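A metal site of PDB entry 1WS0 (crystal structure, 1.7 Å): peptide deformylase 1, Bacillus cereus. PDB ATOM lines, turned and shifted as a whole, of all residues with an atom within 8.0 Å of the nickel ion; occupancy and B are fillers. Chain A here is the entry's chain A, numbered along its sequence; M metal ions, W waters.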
ATOM      1  N   LEU A  14     -28.913 -25.639 -18.530  1.00  0.00           N
ATOM      2  CA  LEU A  14     -27.649 -25.305 -19.198  1.00  0.00           C
ATOM      3  C   LEU A  14     -27.722 -25.260 -20.709  1.00  0.00           C
ATOM      4  O   LEU A  14     -26.902 -24.593 -21.346  1.00  0.00           O
ATOM      5  CB  LEU A  14     -26.553 -26.267 -18.759  1.00  0.00           C
ATOM      6  CG  LEU A  14     -26.169 -26.173 -17.281  1.00  0.00           C
ATOM      7  CD1 LEU A  14     -25.100 -27.231 -16.969  1.00  0.00           C
ATOM      8  CD2 LEU A  14     -25.616 -24.793 -16.962  1.00  0.00           C
ATOM      9  N   GLY A  46     -15.041 -17.135 -15.190  1.00  0.00           N
ATOM     10  CA  GLY A  46     -16.259 -16.740 -15.888  1.00  0.00           C
ATOM     11  C   GLY A  46     -17.466 -17.477 -15.299  1.00  0.00           C
ATOM     12  O   GLY A  46     -17.338 -18.593 -14.755  1.00  0.00           O
ATOM     13  N   LEU A  47     -18.631 -16.840 -15.355  1.00  0.00           N
ATOM     14  CA  LEU A  47     -19.877 -17.456 -14.885  1.00  0.00           C
ATOM     15  C   LEU A  47     -21.025 -16.807 -15.650  1.00  0.00           C
ATOM     16  O   LEU A  47     -21.041 -15.579 -15.823  1.00  0.00           O
ATOM     17  CB  LEU A  47     -20.073 -17.248 -13.373  1.00  0.00           C
ATOM     18  CG  LEU A  47     -21.256 -18.011 -12.754  1.00  0.00           C
ATOM     19  CD1 LEU A  47     -21.005 -19.516 -12.875  1.00  0.00           C
ATOM     20  CD2 LEU A  47     -21.399 -17.642 -11.299  1.00  0.00           C
ATOM     21  N   ALA A  48     -21.978 -17.627 -16.097  1.00  0.00           N
ATOM     22  CA  ALA A  48     -23.147 -17.131 -16.834  1.00  0.00           C
ATOM     23  C   ALA A  48     -24.389 -17.429 -16.021  1.00  0.00           C
ATOM     24  O   ALA A  48     -24.421 -18.414 -15.277  1.00  0.00           O
ATOM     25  CB  ALA A  48     -23.218 -17.837 -18.211  1.00  0.00           C
ATOM     26  N   GLN A  51     -25.978 -20.862 -15.396  1.00  0.00           N
ATOM     27  CA  GLN A  51     -25.250 -21.746 -14.502  1.00  0.00           C
ATOM     28  C   GLN A  51     -25.707 -21.620 -13.081  1.00  0.00           C
ATOM     29  O   GLN A  51     -25.384 -22.457 -12.236  1.00  0.00           O
ATOM     30  CB  GLN A  51     -23.770 -21.484 -14.565  1.00  0.00           C
ATOM     31  CG  GLN A  51     -23.139 -21.803 -15.931  1.00  0.00           C
ATOM     32  CD  GLN A  51     -21.674 -21.551 -15.932  1.00  0.00           C
ATOM     33  OE1 GLN A  51     -21.215 -20.474 -16.323  1.00  0.00           O
ATOM     34  NE2 GLN A  51     -20.907 -22.535 -15.460  1.00  0.00           N
ATOM     35  N   GLU A  88      -9.639 -25.514 -21.955  1.00  0.00           N
ATOM     36  CA  GLU A  88     -10.821 -24.820 -21.472  1.00  0.00           C
ATOM     37  C   GLU A  88     -11.545 -25.690 -20.464  1.00  0.00           C
ATOM     38  O   GLU A  88     -11.615 -26.915 -20.623  1.00  0.00           O
ATOM     39  CB  GLU A  88     -11.739 -24.508 -22.658  1.00  0.00           C
ATOM     40  CG  GLU A  88     -12.311 -23.126 -22.551  1.00  0.00           C
ATOM     41  CD  GLU A  88     -13.189 -22.747 -23.715  1.00  0.00           C
ATOM     42  OE1 GLU A  88     -14.427 -22.959 -23.624  1.00  0.00           O
ATOM     43  OE2 GLU A  88     -12.654 -22.215 -24.707  1.00  0.00           O
ATOM     44  N   GLY A  89     -12.099 -25.055 -19.422  1.00  0.00           N
ATOM     45  CA  GLY A  89     -12.837 -25.753 -18.386  1.00  0.00           C
ATOM     46  C   GLY A  89     -14.127 -25.006 -18.153  1.00  0.00           C
ATOM     47  O   GLY A  89     -14.392 -24.024 -18.858  1.00  0.00           O
ATOM     48  N   CYS A  90     -14.921 -25.442 -17.182  1.00  0.00           N
ATOM     49  CA  CYS A  90     -16.203 -24.801 -16.891  1.00  0.00           C
ATOM     50  C   CYS A  90     -16.635 -25.221 -15.505  1.00  0.00           C
ATOM     51  O   CYS A  90     -16.571 -26.397 -15.188  1.00  0.00           O
ATOM     52  CB  CYS A  90     -17.250 -25.272 -17.890  1.00  0.00           C
ATOM     53  SG  CYS A  90     -18.890 -24.568 -17.652  1.00  0.00           S
ATOM     54  N   LEU A  91     -17.072 -24.269 -14.700  1.00  0.00           N
ATOM     55  CA  LEU A  91     -17.512 -24.610 -13.338  1.00  0.00           C
ATOM     56  C   LEU A  91     -18.672 -25.581 -13.326  1.00  0.00           C
ATOM     57  O   LEU A  91     -18.921 -26.254 -12.314  1.00  0.00           O
ATOM     58  CB  LEU A  91     -17.910 -23.334 -12.541  1.00  0.00           C
ATOM     59  CG  LEU A  91     -16.749 -22.386 -12.216  1.00  0.00           C
ATOM     60  CD1 LEU A  91     -17.301 -21.105 -11.584  1.00  0.00           C
ATOM     61  CD2 LEU A  91     -15.739 -23.068 -11.308  1.00  0.00           C
ATOM     62  N   SER A  92     -19.406 -25.683 -14.430  1.00  0.00           N
ATOM     63  CA  SER A  92     -20.545 -26.608 -14.481  1.00  0.00           C
ATOM     64  C   SER A  92     -20.095 -28.026 -14.804  1.00  0.00           C
ATOM     65  O   SER A  92     -20.912 -28.940 -14.773  1.00  0.00           O
ATOM     66  CB  SER A  92     -21.589 -26.135 -15.502  1.00  0.00           C
ATOM     67  OG  SER A  92     -22.314 -25.028 -14.973  1.00  0.00           O
ATOM     68  N   PHE A  93     -18.808 -28.204 -15.138  1.00  0.00           N
ATOM     69  CA  PHE A  93     -18.268 -29.547 -15.438  1.00  0.00           C
ATOM     70  C   PHE A  93     -17.007 -29.674 -14.593  1.00  0.00           C
ATOM     71  O   PHE A  93     -15.876 -29.599 -15.098  1.00  0.00           O
ATOM     72  CB  PHE A  93     -17.858 -29.690 -16.913  1.00  0.00           C
ATOM     73  CG  PHE A  93     -18.993 -29.578 -17.900  1.00  0.00           C
ATOM     74  CD1 PHE A  93     -19.538 -28.345 -18.215  1.00  0.00           C
ATOM     75  CD2 PHE A  93     -19.467 -30.708 -18.553  1.00  0.00           C
ATOM     76  CE1 PHE A  93     -20.566 -28.239 -19.178  1.00  0.00           C
ATOM     77  CE2 PHE A  93     -20.475 -30.631 -19.509  1.00  0.00           C
ATOM     78  CZ  PHE A  93     -21.034 -29.372 -19.819  1.00  0.00           C
ATOM     79  N   ARG A 102     -10.719 -21.004 -30.187  1.00  0.00           N
ATOM     80  CA  ARG A 102     -11.584 -19.806 -30.101  1.00  0.00           C
ATOM     81  C   ARG A 102     -10.924 -18.697 -30.873  1.00  0.00           C
ATOM     82  O   ARG A 102      -9.745 -18.761 -31.195  1.00  0.00           O
ATOM     83  CB  ARG A 102     -11.657 -19.316 -28.659  1.00  0.00           C
ATOM     84  CG  ARG A 102     -12.227 -20.276 -27.672  1.00  0.00           C
ATOM     85  CD  ARG A 102     -13.734 -20.253 -27.757  1.00  0.00           C
ATOM     86  NE  ARG A 102     -14.333 -21.034 -26.691  1.00  0.00           N
ATOM     87  CZ  ARG A 102     -15.638 -21.270 -26.605  1.00  0.00           C
ATOM     88  NH1 ARG A 102     -16.428 -20.771 -27.545  1.00  0.00           N
ATOM     89  NH2 ARG A 102     -16.132 -21.986 -25.609  1.00  0.00           N
ATOM     90  N   ALA A 129     -12.448 -16.522 -22.344  1.00  0.00           N
ATOM     91  CA  ALA A 129     -13.483 -16.571 -21.317  1.00  0.00           C
ATOM     92  C   ALA A 129     -14.818 -15.945 -21.763  1.00  0.00           C
ATOM     93  O   ALA A 129     -15.912 -16.468 -21.478  1.00  0.00           O
ATOM     94  CB  ALA A 129     -13.001 -15.876 -20.041  1.00  0.00           C
ATOM     95  N   HIS A 132     -16.686 -18.151 -24.191  1.00  0.00           N
ATOM     96  CA  HIS A 132     -17.254 -19.295 -23.491  1.00  0.00           C
ATOM     97  C   HIS A 132     -18.525 -18.863 -22.747  1.00  0.00           C
ATOM     98  O   HIS A 132     -19.563 -19.522 -22.796  1.00  0.00           O
ATOM     99  CB  HIS A 132     -16.177 -19.817 -22.534  1.00  0.00           C
ATOM    100  CG  HIS A 132     -16.654 -20.887 -21.608  1.00  0.00           C
ATOM    101  ND1 HIS A 132     -16.234 -22.189 -21.746  1.00  0.00           N
ATOM    102  CD2 HIS A 132     -17.505 -20.861 -20.559  1.00  0.00           C
ATOM    103  CE1 HIS A 132     -16.811 -22.926 -20.803  1.00  0.00           C
ATOM    104  NE2 HIS A 132     -17.579 -22.148 -20.069  1.00  0.00           N
ATOM    105  N   GLU A 133     -18.467 -17.721 -22.064  1.00  0.00           N
ATOM    106  CA  GLU A 133     -19.665 -17.300 -21.352  1.00  0.00           C
ATOM    107  C   GLU A 133     -20.795 -16.871 -22.259  1.00  0.00           C
ATOM    108  O   GLU A 133     -21.958 -17.130 -21.957  1.00  0.00           O
ATOM    109  CB  GLU A 133     -19.348 -16.174 -20.358  1.00  0.00           C
ATOM    110  CG  GLU A 133     -18.349 -16.578 -19.239  1.00  0.00           C
ATOM    111  CD  GLU A 133     -18.699 -17.917 -18.590  1.00  0.00           C
ATOM    112  OE1 GLU A 133     -19.912 -18.138 -18.351  1.00  0.00           O
ATOM    113  OE2 GLU A 133     -17.772 -18.705 -18.312  1.00  0.00           O
ATOM    114  N   ASP A 135     -21.419 -18.098 -25.148  1.00  0.00           N
ATOM    115  CA  ASP A 135     -22.042 -19.338 -25.606  1.00  0.00           C
ATOM    116  C   ASP A 135     -23.064 -19.827 -24.597  1.00  0.00           C
ATOM    117  O   ASP A 135     -24.146 -20.264 -24.998  1.00  0.00           O
ATOM    118  CB  ASP A 135     -21.028 -20.422 -25.787  1.00  0.00           C
ATOM    119  CG  ASP A 135     -20.302 -20.335 -27.118  1.00  0.00           C
ATOM    120  OD1 ASP A 135     -20.630 -19.474 -27.963  1.00  0.00           O
ATOM    121  OD2 ASP A 135     -19.402 -21.160 -27.319  1.00  0.00           O
ATOM    122  N   HIS A 136     -22.744 -19.790 -23.305  1.00  0.00           N
ATOM    123  CA  HIS A 136     -23.733 -20.240 -22.278  1.00  0.00           C
ATOM    124  C   HIS A 136     -25.086 -19.529 -22.423  1.00  0.00           C
ATOM    125  O   HIS A 136     -26.161 -20.133 -22.193  1.00  0.00           O
ATOM    126  CB  HIS A 136     -23.261 -19.913 -20.865  1.00  0.00           C
ATOM    127  CG  HIS A 136     -22.372 -20.951 -20.242  1.00  0.00           C
ATOM    128  ND1 HIS A 136     -22.815 -22.220 -19.967  1.00  0.00           N
ATOM    129  CD2 HIS A 136     -21.094 -20.889 -19.813  1.00  0.00           C
ATOM    130  CE1 HIS A 136     -21.844 -22.906 -19.391  1.00  0.00           C
ATOM    131  NE2 HIS A 136     -20.783 -22.118 -19.295  1.00  0.00           N
ATOM    132  N   VAL A 140     -25.275 -23.002 -25.357  1.00  0.00           N
ATOM    133  CA  VAL A 140     -24.166 -23.786 -25.907  1.00  0.00           C
ATOM    134  C   VAL A 140     -23.097 -24.033 -24.856  1.00  0.00           C
ATOM    135  O   VAL A 140     -22.631 -23.102 -24.195  1.00  0.00           O
ATOM    136  CB  VAL A 140     -23.506 -23.032 -27.101  1.00  0.00           C
ATOM    137  CG1 VAL A 140     -22.253 -23.799 -27.655  1.00  0.00           C
ATOM    138  CG2 VAL A 140     -24.538 -22.879 -28.212  1.00  0.00           C
ATOM    139  N   LEU A 141     -22.693 -25.299 -24.730  1.00  0.00           N
ATOM    140  CA  LEU A 141     -21.688 -25.713 -23.740  1.00  0.00           C
ATOM    141  C   LEU A 141     -20.367 -26.040 -24.441  1.00  0.00           C
ATOM    142  O   LEU A 141     -20.341 -26.502 -25.590  1.00  0.00           O
ATOM    143  CB  LEU A 141     -22.229 -26.934 -22.960  1.00  0.00           C
ATOM    144  CG  LEU A 141     -23.600 -26.646 -22.309  1.00  0.00           C
ATOM    145  CD1 LEU A 141     -24.138 -27.877 -21.582  1.00  0.00           C
ATOM    146  CD2 LEU A 141     -23.456 -25.497 -21.317  1.00  0.00           C
ATOM    147  N   PHE A 142     -19.252 -25.846 -23.738  1.00  0.00           N
ATOM    148  CA  PHE A 142     -17.968 -26.021 -24.364  1.00  0.00           C
ATOM    149  C   PHE A 142     -17.676 -27.421 -24.886  1.00  0.00           C
ATOM    150  O   PHE A 142     -16.865 -27.591 -25.798  1.00  0.00           O
ATOM    151  CB  PHE A 142     -16.851 -25.518 -23.440  1.00  0.00           C
ATOM    152  CG  PHE A 142     -16.391 -26.490 -22.423  1.00  0.00           C
ATOM    153  CD1 PHE A 142     -15.082 -26.960 -22.454  1.00  0.00           C
ATOM    154  CD2 PHE A 142     -17.258 -26.943 -21.427  1.00  0.00           C
ATOM    155  CE1 PHE A 142     -14.634 -27.886 -21.476  1.00  0.00           C
ATOM    156  CE2 PHE A 142     -16.825 -27.865 -20.457  1.00  0.00           C
ATOM    157  CZ  PHE A 142     -15.511 -28.330 -20.481  1.00  0.00           C
HETATM  158 NI    NI M   1     -18.894 -22.508 -18.540  1.00  0.00          NI
HETATM  159  O   HOH W   1     -18.722 -20.813 -17.320  1.00  0.00           O
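The nickel ion is bound by NE2 of His 132, at 2.0 Å. The nickel ion is bound by NE2 of His 136 (2.1 Å). Water W1 binds the nickel ion, 2.1 Å away. SG of Cys 90 is bound to the nickel ion (2.2 Å). The nickel ion has four donor atoms within binding distance.
Water W1 lies within hydrogen-bond range of OE2 of Glu 133 and OE1 of Gln 51.
A ring nitrogen (ND1) of His 132 sits at hydrogen-bond distance from the side-chain carboxylate (OE1) of Glu 88 (2.7 Å). A ring nitrogen (NE2) of His 136 sits close to the side-chain amide oxygen of Gln 51, at 3.4 Å. The side-chain amide nitrogen (NE2) of Gln 51 sits close to the side-chain sulfur (SG) of Cys 90, 3.6 Å away. The side-chain sulfur of Cys 90 lies close to the backbone NH of Ser 92, 3.4 Å away. The side-chain amide oxygen (OE1) of Gln 51 sits close to the side-chain carboxylate (OE1) of Glu 133, 3.4 Å away. OG of Ser 92 sits at hydrogen-bond distance from NE2 of Gln 51, 2.9 Å away. The backbone NH (N) of Ala 48 is in hydrogen-bond range of the side-chain amide oxygen (OE1) of Gln 51, 3.0 Å away. The side-chain carboxylate (OE1) of Glu 133 lies within hydrogen-bond range of the backbone NH (N) of Ala 48.
Merely in contact with the nickel ion: Gln 51 (3.7 Å) and Glu 133 (3.97 Å). Five residues have an atom within 4 Å of the nickel ion: Gln 51, Cys 90, His 132, Glu 133 and His 136. The nearest printed residue that does not touch the nickel ion is Leu 91 (4.6 Å).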
